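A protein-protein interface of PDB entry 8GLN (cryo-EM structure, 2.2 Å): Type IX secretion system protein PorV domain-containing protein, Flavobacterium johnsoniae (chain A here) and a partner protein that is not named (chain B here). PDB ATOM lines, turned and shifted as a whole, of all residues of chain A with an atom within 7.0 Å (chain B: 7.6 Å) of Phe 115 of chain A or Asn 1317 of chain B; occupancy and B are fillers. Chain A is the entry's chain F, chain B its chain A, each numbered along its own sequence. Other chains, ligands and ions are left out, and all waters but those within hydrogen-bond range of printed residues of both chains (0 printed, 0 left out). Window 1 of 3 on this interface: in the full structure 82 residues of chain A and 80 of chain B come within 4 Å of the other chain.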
ATOM      1  N   VAL A  30     -22.209 -25.796  14.975  1.00  0.00           N
ATOM      2  CA  VAL A  30     -20.878 -26.405  14.861  1.00  0.00           C
ATOM      3  C   VAL A  30     -20.055 -25.755  13.752  1.00  0.00           C
ATOM      4  O   VAL A  30     -19.722 -26.416  12.758  1.00  0.00           O
ATOM      5  CB  VAL A  30     -20.963 -27.933  14.675  1.00  0.00           C
ATOM      6  CG1 VAL A  30     -21.262 -28.607  16.003  1.00  0.00           C
ATOM      7  CG2 VAL A  30     -22.006 -28.338  13.634  1.00  0.00           C
ATOM      8  N   PRO A  31     -19.693 -24.475  13.881  1.00  0.00           N
ATOM      9  CA  PRO A  31     -18.933 -23.815  12.807  1.00  0.00           C
ATOM     10  C   PRO A  31     -17.511 -24.330  12.658  1.00  0.00           C
ATOM     11  O   PRO A  31     -16.844 -23.963  11.683  1.00  0.00           O
ATOM     12  CB  PRO A  31     -18.947 -22.333  13.211  1.00  0.00           C
ATOM     13  CG  PRO A  31     -19.520 -22.268  14.597  1.00  0.00           C
ATOM     14  CD  PRO A  31     -19.785 -23.648  15.095  1.00  0.00           C
ATOM     15  N   PHE A  32     -17.030 -25.162  13.584  1.00  0.00           N
ATOM     16  CA  PHE A  32     -15.695 -25.736  13.459  1.00  0.00           C
ATOM     17  C   PHE A  32     -15.568 -26.668  12.261  1.00  0.00           C
ATOM     18  O   PHE A  32     -14.445 -26.976  11.850  1.00  0.00           O
ATOM     19  CB  PHE A  32     -15.320 -26.475  14.747  1.00  0.00           C
ATOM     20  CG  PHE A  32     -15.742 -27.920  14.769  1.00  0.00           C
ATOM     21  CD1 PHE A  32     -17.038 -28.270  15.111  1.00  0.00           C
ATOM     22  CD2 PHE A  32     -14.840 -28.927  14.468  1.00  0.00           C
ATOM     23  CE1 PHE A  32     -17.429 -29.595  15.138  1.00  0.00           C
ATOM     24  CE2 PHE A  32     -15.226 -30.254  14.495  1.00  0.00           C
ATOM     25  CZ  PHE A  32     -16.521 -30.587  14.830  1.00  0.00           C
ATOM     26  N   TYR A  81      -4.442 -23.022  17.908  1.00  0.00           N
ATOM     27  CA  TYR A  81      -5.184 -21.788  18.113  1.00  0.00           C
ATOM     28  C   TYR A  81      -4.556 -21.001  19.253  1.00  0.00           C
ATOM     29  O   TYR A  81      -4.136 -21.584  20.258  1.00  0.00           O
ATOM     30  CB  TYR A  81      -6.655 -22.065  18.440  1.00  0.00           C
ATOM     31  CG  TYR A  81      -7.514 -22.377  17.240  1.00  0.00           C
ATOM     32  CD1 TYR A  81      -7.474 -23.626  16.637  1.00  0.00           C
ATOM     33  CD2 TYR A  81      -8.376 -21.424  16.715  1.00  0.00           C
ATOM     34  CE1 TYR A  81      -8.262 -23.915  15.542  1.00  0.00           C
ATOM     35  CE2 TYR A  81      -9.168 -21.704  15.621  1.00  0.00           C
ATOM     36  CZ  TYR A  81      -9.107 -22.950  15.039  1.00  0.00           C
ATOM     37  OH  TYR A  81      -9.894 -23.233  13.949  1.00  0.00           O
ATOM     38  N   LEU A  82      -4.506 -19.678  19.094  1.00  0.00           N
ATOM     39  CA  LEU A  82      -3.995 -18.772  20.124  1.00  0.00           C
ATOM     40  C   LEU A  82      -2.616 -19.213  20.606  1.00  0.00           C
ATOM     41  O   LEU A  82      -2.372 -19.390  21.802  1.00  0.00           O
ATOM     42  CB  LEU A  82      -4.977 -18.667  21.291  1.00  0.00           C
ATOM     43  CG  LEU A  82      -6.447 -18.455  20.926  1.00  0.00           C
ATOM     44  CD1 LEU A  82      -7.345 -18.792  22.105  1.00  0.00           C
ATOM     45  CD2 LEU A  82      -6.686 -17.028  20.457  1.00  0.00           C
ATOM     46  N   ASN A  87      -0.995 -23.082  24.870  1.00  0.00           N
ATOM     47  CA  ASN A  87      -0.759 -24.290  24.096  1.00  0.00           C
ATOM     48  C   ASN A  87      -1.932 -25.248  24.260  1.00  0.00           C
ATOM     49  O   ASN A  87      -2.825 -25.045  25.085  1.00  0.00           O
ATOM     50  CB  ASN A  87       0.547 -24.967  24.527  1.00  0.00           C
ATOM     51  CG  ASN A  87       1.723 -24.574  23.659  1.00  0.00           C
ATOM     52  OD1 ASN A  87       1.576 -23.823  22.695  1.00  0.00           O
ATOM     53  ND2 ASN A  87       2.901 -25.085  23.994  1.00  0.00           N
ATOM     54  N   ASP A  88      -1.918 -26.301  23.443  1.00  0.00           N
ATOM     55  CA  ASP A  88      -2.880 -27.400  23.464  1.00  0.00           C
ATOM     56  C   ASP A  88      -4.293 -26.973  23.087  1.00  0.00           C
ATOM     57  O   ASP A  88      -5.237 -27.742  23.299  1.00  0.00           O
ATOM     58  CB  ASP A  88      -2.906 -28.105  24.826  1.00  0.00           C
ATOM     59  CG  ASP A  88      -1.658 -28.925  25.079  1.00  0.00           C
ATOM     60  OD1 ASP A  88      -1.469 -29.947  24.387  1.00  0.00           O
ATOM     61  OD2 ASP A  88      -0.864 -28.549  25.967  1.00  0.00           O
ATOM     62  N   ILE A  89      -4.470 -25.777  22.540  1.00  0.00           N
ATOM     63  CA  ILE A  89      -5.731 -25.362  21.940  1.00  0.00           C
ATOM     64  C   ILE A  89      -5.563 -25.493  20.434  1.00  0.00           C
ATOM     65  O   ILE A  89      -4.920 -24.652  19.797  1.00  0.00           O
ATOM     66  CB  ILE A  89      -6.114 -23.931  22.334  1.00  0.00           C
ATOM     67  CG1 ILE A  89      -6.066 -23.762  23.853  1.00  0.00           C
ATOM     68  CG2 ILE A  89      -7.490 -23.582  21.790  1.00  0.00           C
ATOM     69  CD1 ILE A  89      -6.441 -22.376  24.319  1.00  0.00           C
ATOM     70  N   SER A  90      -6.132 -26.546  19.856  1.00  0.00           N
ATOM     71  CA  SER A  90      -5.841 -26.855  18.467  1.00  0.00           C
ATOM     72  C   SER A  90      -6.987 -27.633  17.844  1.00  0.00           C
ATOM     73  O   SER A  90      -7.852 -28.177  18.535  1.00  0.00           O
ATOM     74  CB  SER A  90      -4.538 -27.649  18.337  1.00  0.00           C
ATOM     75  OG  SER A  90      -4.740 -29.014  18.653  1.00  0.00           O
ATOM     76  N   TYR A 112     -11.033 -33.069  15.326  1.00  0.00           N
ATOM     77  CA  TYR A 112     -11.172 -32.898  16.766  1.00  0.00           C
ATOM     78  C   TYR A 112     -10.659 -31.524  17.160  1.00  0.00           C
ATOM     79  O   TYR A 112      -9.475 -31.227  16.978  1.00  0.00           O
ATOM     80  CB  TYR A 112     -10.414 -33.997  17.519  1.00  0.00           C
ATOM     81  CG  TYR A 112     -10.593 -33.980  19.020  1.00  0.00           C
ATOM     82  CD1 TYR A 112      -9.824 -33.149  19.824  1.00  0.00           C
ATOM     83  CD2 TYR A 112     -11.523 -34.806  19.634  1.00  0.00           C
ATOM     84  CE1 TYR A 112      -9.983 -33.135  21.193  1.00  0.00           C
ATOM     85  CE2 TYR A 112     -11.688 -34.800  21.003  1.00  0.00           C
ATOM     86  CZ  TYR A 112     -10.916 -33.964  21.778  1.00  0.00           C
ATOM     87  OH  TYR A 112     -11.077 -33.955  23.143  1.00  0.00           O
ATOM     88  N   PHE A 113     -11.543 -30.694  17.703  1.00  0.00           N
ATOM     89  CA  PHE A 113     -11.173 -29.405  18.271  1.00  0.00           C
ATOM     90  C   PHE A 113     -11.314 -29.491  19.782  1.00  0.00           C
ATOM     91  O   PHE A 113     -12.389 -29.825  20.289  1.00  0.00           O
ATOM     92  CB  PHE A 113     -12.040 -28.275  17.714  1.00  0.00           C
ATOM     93  CG  PHE A 113     -11.786 -26.945  18.364  1.00  0.00           C
ATOM     94  CD1 PHE A 113     -10.763 -26.126  17.916  1.00  0.00           C
ATOM     95  CD2 PHE A 113     -12.564 -26.515  19.426  1.00  0.00           C
ATOM     96  CE1 PHE A 113     -10.522 -24.906  18.513  1.00  0.00           C
ATOM     97  CE2 PHE A 113     -12.327 -25.296  20.027  1.00  0.00           C
ATOM     98  CZ  PHE A 113     -11.304 -24.490  19.569  1.00  0.00           C
ATOM     99  N   GLY A 114     -10.234 -29.187  20.498  1.00  0.00           N
ATOM    100  CA  GLY A 114     -10.252 -29.252  21.942  1.00  0.00           C
ATOM    101  C   GLY A 114      -9.325 -28.216  22.543  1.00  0.00           C
ATOM    102  O   GLY A 114      -8.395 -27.727  21.899  1.00  0.00           O
ATOM    103  N   PHE A 115      -9.600 -27.888  23.803  1.00  0.00           N
ATOM    104  CA  PHE A 115      -8.785 -26.961  24.569  1.00  0.00           C
ATOM    105  C   PHE A 115      -7.770 -27.676  25.448  1.00  0.00           C
ATOM    106  O   PHE A 115      -7.067 -27.024  26.223  1.00  0.00           O
ATOM    107  CB  PHE A 115      -9.676 -26.063  25.425  1.00  0.00           C
ATOM    108  CG  PHE A 115     -10.684 -25.289  24.636  1.00  0.00           C
ATOM    109  CD1 PHE A 115     -10.307 -24.173  23.912  1.00  0.00           C
ATOM    110  CD2 PHE A 115     -12.009 -25.681  24.611  1.00  0.00           C
ATOM    111  CE1 PHE A 115     -11.233 -23.463  23.180  1.00  0.00           C
ATOM    112  CE2 PHE A 115     -12.941 -24.974  23.883  1.00  0.00           C
ATOM    113  CZ  PHE A 115     -12.552 -23.864  23.165  1.00  0.00           C
ATOM    114  N   GLY A 116      -7.682 -28.995  25.344  1.00  0.00           N
ATOM    115  CA  GLY A 116      -6.853 -29.768  26.245  1.00  0.00           C
ATOM    116  C   GLY A 116      -7.518 -29.916  27.601  1.00  0.00           C
ATOM    117  O   GLY A 116      -8.609 -29.410  27.860  1.00  0.00           O
ATOM    118  N   GLY A 117      -6.833 -30.638  28.482  1.00  0.00           N
ATOM    119  CA  GLY A 117      -7.338 -30.815  29.833  1.00  0.00           C
ATOM    120  C   GLY A 117      -7.321 -29.501  30.591  1.00  0.00           C
ATOM    121  O   GLY A 117      -6.321 -28.774  30.583  1.00  0.00           O
ATOM    122  N   ILE A 118      -8.433 -29.186  31.246  1.00  0.00           N
ATOM    123  CA  ILE A 118      -8.547 -28.005  32.093  1.00  0.00           C
ATOM    124  C   ILE A 118      -8.886 -28.473  33.499  1.00  0.00           C
ATOM    125  O   ILE A 118      -9.861 -29.208  33.696  1.00  0.00           O
ATOM    126  CB  ILE A 118      -9.605 -27.018  31.574  1.00  0.00           C
ATOM    127  CG1 ILE A 118      -9.351 -26.685  30.103  1.00  0.00           C
ATOM    128  CG2 ILE A 118      -9.613 -25.758  32.421  1.00  0.00           C
ATOM    129  CD1 ILE A 118     -10.514 -26.004  29.426  1.00  0.00           C
ATOM    130  N   VAL A 133     -11.704 -31.331  33.046  1.00  0.00           N
ATOM    131  CA  VAL A 133     -12.628 -31.333  31.922  1.00  0.00           C
ATOM    132  C   VAL A 133     -11.850 -31.022  30.653  1.00  0.00           C
ATOM    133  O   VAL A 133     -10.860 -30.285  30.670  1.00  0.00           O
ATOM    134  CB  VAL A 133     -13.784 -30.328  32.116  1.00  0.00           C
ATOM    135  CG1 VAL A 133     -14.611 -30.711  33.327  1.00  0.00           C
ATOM    136  CG2 VAL A 133     -13.246 -28.915  32.261  1.00  0.00           C
ATOM    137  N   ASN A 134     -12.299 -31.607  29.548  1.00  0.00           N
ATOM    138  CA  ASN A 134     -11.720 -31.363  28.230  1.00  0.00           C
ATOM    139  C   ASN A 134     -12.849 -30.970  27.287  1.00  0.00           C
ATOM    140  O   ASN A 134     -13.370 -31.802  26.532  1.00  0.00           O
ATOM    141  CB  ASN A 134     -10.929 -32.579  27.736  1.00  0.00           C
ATOM    142  CG  ASN A 134     -11.772 -33.837  27.647  1.00  0.00           C
ATOM    143  OD1 ASN A 134     -12.521 -34.164  28.566  1.00  0.00           O
ATOM    144  ND2 ASN A 134     -11.650 -34.551  26.534  1.00  0.00           N
ATOM    145  N   PRO A 135     -13.271 -29.706  27.321  1.00  0.00           N
ATOM    146  CA  PRO A 135     -14.281 -29.245  26.361  1.00  0.00           C
ATOM    147  C   PRO A 135     -13.777 -29.446  24.942  1.00  0.00           C
ATOM    148  O   PRO A 135     -12.642 -29.097  24.612  1.00  0.00           O
ATOM    149  CB  PRO A 135     -14.451 -27.760  26.701  1.00  0.00           C
ATOM    150  CG  PRO A 135     -13.880 -27.595  28.065  1.00  0.00           C
ATOM    151  CD  PRO A 135     -12.814 -28.628  28.212  1.00  0.00           C
ATOM    152  N   ASN A 136     -14.628 -30.019  24.100  1.00  0.00           N
ATOM    153  CA  ASN A 136     -14.164 -30.418  22.783  1.00  0.00           C
ATOM    154  C   ASN A 136     -15.341 -30.533  21.830  1.00  0.00           C
ATOM    155  O   ASN A 136     -16.500 -30.614  22.241  1.00  0.00           O
ATOM    156  CB  ASN A 136     -13.395 -31.741  22.841  1.00  0.00           C
ATOM    157  CG  ASN A 136     -14.270 -32.907  23.253  1.00  0.00           C
ATOM    158  OD1 ASN A 136     -14.782 -33.640  22.408  1.00  0.00           O
ATOM    159  ND2 ASN A 136     -14.444 -33.085  24.555  1.00  0.00           N
ATOM    160  N   GLU A 137     -15.011 -30.531  20.544  1.00  0.00           N
ATOM    161  CA  GLU A 137     -15.953 -30.780  19.465  1.00  0.00           C
ATOM    162  C   GLU A 137     -15.256 -31.693  18.473  1.00  0.00           C
ATOM    163  O   GLU A 137     -14.093 -31.456  18.134  1.00  0.00           O
ATOM    164  CB  GLU A 137     -16.378 -29.474  18.782  1.00  0.00           C
ATOM    165  CG  GLU A 137     -17.696 -28.910  19.264  1.00  0.00           C
ATOM    166  CD  GLU A 137     -17.987 -27.533  18.694  1.00  0.00           C
ATOM    167  OE1 GLU A 137     -19.166 -27.251  18.390  1.00  0.00           O
ATOM    168  OE2 GLU A 137     -17.038 -26.735  18.550  1.00  0.00           O
ATOM    169  N   LEU A 165     -18.662 -28.568  24.273  1.00  0.00           N
ATOM    170  CA  LEU A 165     -17.882 -27.429  24.738  1.00  0.00           C
ATOM    171  C   LEU A 165     -18.307 -26.935  26.114  1.00  0.00           C
ATOM    172  O   LEU A 165     -17.514 -26.271  26.789  1.00  0.00           O
ATOM    173  CB  LEU A 165     -17.981 -26.282  23.731  1.00  0.00           C
ATOM    174  CG  LEU A 165     -17.428 -26.558  22.331  1.00  0.00           C
ATOM    175  CD1 LEU A 165     -17.507 -25.309  21.472  1.00  0.00           C
ATOM    176  CD2 LEU A 165     -15.999 -27.068  22.410  1.00  0.00           C
ATOM    177  N   PRO A 382      -8.306 -15.752  13.873  1.00  0.00           N
ATOM    178  CA  PRO A 382      -7.720 -16.524  14.981  1.00  0.00           C
ATOM    179  C   PRO A 382      -6.547 -17.395  14.566  1.00  0.00           C
ATOM    180  O   PRO A 382      -5.764 -17.804  15.430  1.00  0.00           O
ATOM    181  CB  PRO A 382      -8.902 -17.368  15.477  1.00  0.00           C
ATOM    182  CG  PRO A 382      -9.777 -17.502  14.270  1.00  0.00           C
ATOM    183  CD  PRO A 382      -9.696 -16.158  13.603  1.00  0.00           C
ATOM    184  N   ILE B 949     -24.002 -14.789  20.890  1.00  0.00           N
ATOM    185  CA  ILE B 949     -23.460 -15.875  21.698  1.00  0.00           C
ATOM    186  C   ILE B 949     -22.763 -16.858  20.771  1.00  0.00           C
ATOM    187  O   ILE B 949     -23.317 -17.240  19.734  1.00  0.00           O
ATOM    188  CB  ILE B 949     -24.559 -16.581  22.513  1.00  0.00           C
ATOM    189  CG1 ILE B 949     -25.243 -15.594  23.453  1.00  0.00           C
ATOM    190  CG2 ILE B 949     -23.979 -17.749  23.294  1.00  0.00           C
ATOM    191  CD1 ILE B 949     -26.586 -16.062  23.921  1.00  0.00           C
ATOM    192  N   ALA B 950     -21.550 -17.259  21.142  1.00  0.00           N
ATOM    193  CA  ALA B 950     -20.818 -18.239  20.354  1.00  0.00           C
ATOM    194  C   ALA B 950     -21.575 -19.559  20.306  1.00  0.00           C
ATOM    195  O   ALA B 950     -22.177 -19.988  21.295  1.00  0.00           O
ATOM    196  CB  ALA B 950     -19.421 -18.452  20.938  1.00  0.00           C
ATOM    197  N   GLN B 951     -21.551 -20.199  19.140  1.00  0.00           N
ATOM    198  CA  GLN B 951     -22.242 -21.469  18.970  1.00  0.00           C
ATOM    199  C   GLN B 951     -21.611 -22.539  19.853  1.00  0.00           C
ATOM    200  O   GLN B 951     -20.386 -22.636  19.962  1.00  0.00           O
ATOM    201  CB  GLN B 951     -22.201 -21.900  17.504  1.00  0.00           C
ATOM    202  CG  GLN B 951     -22.801 -20.882  16.551  1.00  0.00           C
ATOM    203  CD  GLN B 951     -24.271 -20.630  16.819  1.00  0.00           C
ATOM    204  OE1 GLN B 951     -24.701 -19.488  16.964  1.00  0.00           O
ATOM    205  NE2 GLN B 951     -25.051 -21.702  16.886  1.00  0.00           N
ATOM    206  N   GLY B 952     -22.459 -23.344  20.486  1.00  0.00           N
ATOM    207  CA  GLY B 952     -22.007 -24.341  21.429  1.00  0.00           C
ATOM    208  C   GLY B 952     -21.850 -23.852  22.851  1.00  0.00           C
ATOM    209  O   GLY B 952     -21.545 -24.661  23.735  1.00  0.00           O
ATOM    210  N   GLN B 953     -22.045 -22.562  23.099  1.00  0.00           N
ATOM    211  CA  GLN B 953     -21.936 -21.988  24.427  1.00  0.00           C
ATOM    212  C   GLN B 953     -23.319 -21.911  25.073  1.00  0.00           C
ATOM    213  O   GLN B 953     -24.299 -22.465  24.568  1.00  0.00           O
ATOM    214  CB  GLN B 953     -21.259 -20.618  24.350  1.00  0.00           C
ATOM    215  CG  GLN B 953     -19.741 -20.676  24.313  1.00  0.00           C
ATOM    216  CD  GLN B 953     -19.175 -21.803  25.156  1.00  0.00           C
ATOM    217  OE1 GLN B 953     -18.594 -22.753  24.632  1.00  0.00           O
ATOM    218  NE2 GLN B 953     -19.337 -21.700  26.470  1.00  0.00           N
ATOM    219  N   LEU B1314     -15.651  -9.515  16.713  1.00  0.00           N
ATOM    220  CA  LEU B1314     -14.591 -10.455  17.049  1.00  0.00           C
ATOM    221  C   LEU B1314     -15.037 -11.875  16.729  1.00  0.00           C
ATOM    222  O   LEU B1314     -16.229 -12.166  16.606  1.00  0.00           O
ATOM    223  CB  LEU B1314     -14.196 -10.358  18.531  1.00  0.00           C
ATOM    224  CG  LEU B1314     -13.787  -8.983  19.058  1.00  0.00           C
ATOM    225  CD1 LEU B1314     -13.537  -9.038  20.555  1.00  0.00           C
ATOM    226  CD2 LEU B1314     -12.552  -8.479  18.331  1.00  0.00           C
ATOM    227  N   TYR B1315     -14.053 -12.762  16.592  1.00  0.00           N
ATOM    228  CA  TYR B1315     -14.287 -14.188  16.382  1.00  0.00           C
ATOM    229  C   TYR B1315     -14.134 -14.896  17.722  1.00  0.00           C
ATOM    230  O   TYR B1315     -13.063 -14.852  18.332  1.00  0.00           O
ATOM    231  CB  TYR B1315     -13.307 -14.751  15.355  1.00  0.00           C
ATOM    232  CG  TYR B1315     -13.745 -14.590  13.919  1.00  0.00           C
ATOM    233  CD1 TYR B1315     -14.919 -15.173  13.462  1.00  0.00           C
ATOM    234  CD2 TYR B1315     -12.988 -13.851  13.021  1.00  0.00           C
ATOM    235  CE1 TYR B1315     -15.321 -15.031  12.151  1.00  0.00           C
ATOM    236  CE2 TYR B1315     -13.385 -13.700  11.707  1.00  0.00           C
ATOM    237  CZ  TYR B1315     -14.553 -14.291  11.278  1.00  0.00           C
ATOM    238  OH  TYR B1315     -14.953 -14.144   9.971  1.00  0.00           O
ATOM    239  N   ASN B1316     -15.200 -15.557  18.179  1.00  0.00           N
ATOM    240  CA  ASN B1316     -15.134 -16.245  19.465  1.00  0.00           C
ATOM    241  C   ASN B1316     -14.742 -17.707  19.286  1.00  0.00           C
ATOM    242  O   ASN B1316     -13.696 -18.146  19.777  1.00  0.00           O
ATOM    243  CB  ASN B1316     -16.474 -16.127  20.194  1.00  0.00           C
ATOM    244  CG  ASN B1316     -16.328 -16.208  21.699  1.00  0.00           C
ATOM    245  OD1 ASN B1316     -16.615 -15.251  22.415  1.00  0.00           O
ATOM    246  ND2 ASN B1316     -15.876 -17.357  22.187  1.00  0.00           N
ATOM    247  N   ASN B1317     -15.576 -18.483  18.590  1.00  0.00           N
ATOM    248  CA  ASN B1317     -15.203 -19.822  18.119  1.00  0.00           C
ATOM    249  C   ASN B1317     -15.778 -19.959  16.712  1.00  0.00           C
ATOM    250  O   ASN B1317     -16.889 -20.467  16.536  1.00  0.00           O
ATOM    251  CB  ASN B1317     -15.710 -20.926  19.042  1.00  0.00           C
ATOM    252  CG  ASN B1317     -15.628 -20.554  20.511  1.00  0.00           C
ATOM    253  OD1 ASN B1317     -16.326 -19.656  20.977  1.00  0.00           O
ATOM    254  ND2 ASN B1317     -14.770 -21.249  21.249  1.00  0.00           N
ATOM    255  N   ASN B1318     -15.008 -19.520  15.717  1.00  0.00           N
ATOM    256  CA  ASN B1318     -15.419 -19.539  14.310  1.00  0.00           C
ATOM    257  C   ASN B1318     -16.758 -18.836  14.087  1.00  0.00           C
ATOM    258  O   ASN B1318     -17.440 -19.090  13.089  1.00  0.00           O
ATOM    259  CB  ASN B1318     -15.473 -20.971  13.769  1.00  0.00           C
ATOM    260  CG  ASN B1318     -14.327 -21.826  14.272  1.00  0.00           C
ATOM    261  OD1 ASN B1318     -13.166 -21.575  13.952  1.00  0.00           O
ATOM    262  ND2 ASN B1318     -14.649 -22.837  15.068  1.00  0.00           N
ATOM    263  N   THR B1319     -17.150 -17.951  15.000  1.00  0.00           N
ATOM    264  CA  THR B1319     -18.404 -17.216  14.898  1.00  0.00           C
ATOM    265  C   THR B1319     -18.152 -15.738  15.154  1.00  0.00           C
ATOM    266  O   THR B1319     -17.339 -15.375  16.009  1.00  0.00           O
ATOM    267  CB  THR B1319     -19.454 -17.752  15.886  1.00  0.00           C
ATOM    268  OG1 THR B1319     -20.621 -16.923  15.845  1.00  0.00           O
ATOM    269  CG2 THR B1319     -18.900 -17.778  17.302  1.00  0.00           C
ATOM    270  N   VAL B1320     -18.844 -14.890  14.400  1.00  0.00           N
ATOM    271  CA  VAL B1320     -18.703 -13.446  14.549  1.00  0.00           C
ATOM    272  C   VAL B1320     -19.545 -12.986  15.730  1.00  0.00           C
ATOM    273  O   VAL B1320     -20.747 -13.265  15.798  1.00  0.00           O
ATOM    274  CB  VAL B1320     -19.119 -12.722  13.259  1.00  0.00           C
ATOM    275  CG1 VAL B1320     -19.076 -11.214  13.460  1.00  0.00           C
ATOM    276  CG2 VAL B1320     -18.223 -13.131  12.105  1.00  0.00           C
ATOM    277  N   ILE B1321     -18.916 -12.278  16.662  1.00  0.00           N
ATOM    278  CA  ILE B1321     -19.591 -11.742  17.838  1.00  0.00           C
ATOM    279  C   ILE B1321     -19.542 -10.224  17.757  1.00  0.00           C
ATOM    280  O   ILE B1321     -18.456  -9.632  17.744  1.00  0.00           O
ATOM    281  CB  ILE B1321     -18.951 -12.241  19.143  1.00  0.00           C
ATOM    282  CG1 ILE B1321     -18.978 -13.769  19.202  1.00  0.00           C
ATOM    283  CG2 ILE B1321     -19.656 -11.639  20.348  1.00  0.00           C
ATOM    284  CD1 ILE B1321     -20.365 -14.356  19.302  1.00  0.00           C
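The side-chain amide oxygen (OD1) of Asn 1317 of chain B is in hydrogen-bond range of the side-chain amide nitrogen (ND2) of Asn 1316 of chain B (2.6 Å). The backbone NH (N) of Phe 115 of chain A sits at hydrogen-bond distance from the backbone carbonyl oxygen (O) of Pro 135 of chain A (3.4 Å). The backbone NH (N) of Tyr 81 of chain A sits at hydrogen-bond distance from the backbone carbonyl oxygen (O) of Ile 89 of chain A, 2.5 Å away.
Pro 31 of chain A touches Gln 951 of chain B (CD to CB, 3.8 Å). Asn 1317 of chain B touches Pro 31 of chain A. CB of Pro 31 of chain A touches O of Asn 1318 of chain B, 3.6 Å away. Asn 1318 of chain B touches Phe 32 of chain A (ND2 to CA, 3.5 Å). Tyr 81 of chain A touches Asn 1318 of chain B (OH to OD1, 3.7 Å). CZ of Phe 115 of chain A touches ND2 of Asn 1317 of chain B (3.9 Å). Leu 165 of chain A touches Gly 952 of chain B (CB to O, 3.9 Å). Leu 165 of chain A touches Gln 953 of chain B (CB to OE1, 3.7 Å).
Of the printed residues of chain B, Pro 31 of chain A touches Gln 951 (3.8 Å), Asn 1317 (3.7 Å) and Asn 1318 (3.6 Å). Asn 87 of chain A touches none of the printed residues of chain B. Of chain B, only Asn 1317 (3.9 Å) comes within 4 Å of Phe 115 of chain A. No residue of chain B comes within 4 Å of Gly 116 of chain A. Printed residues of chain A within 4 Å of Gln 951 of chain B: Pro 31 (3.8 Å). Of the printed residues of chain A, Gly 952 of chain B touches Leu 165 (3.9 Å). Of chain A, only Pro 31 (3.7 Å) and Phe 115 (3.9 Å) come within 4 Å of Asn 1317 of chain B. Printed residues of chain A within 4 Å of Asn 1318 of chain B: Pro 31, Phe 32 and Tyr 81. The nearest printed residue of chain A that does not touch Gln 953 of chain B is Phe 115 of chain A (6.1 Å).
Hydrophobic or aromatic side chains of chain A that line the printed part of chain B: Pro 31, Phe 32, Tyr 81, Phe 115 and Leu 165. Of the 13 printed residues of chain B, 5 touch a printed residue of chain A. Among the printed residues, 8 pairs touch across the chains. Among the printed residues, no Asp or Glu carboxylate lies within 4 Å of a Lys or Arg side-chain nitrogen of the other chain.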
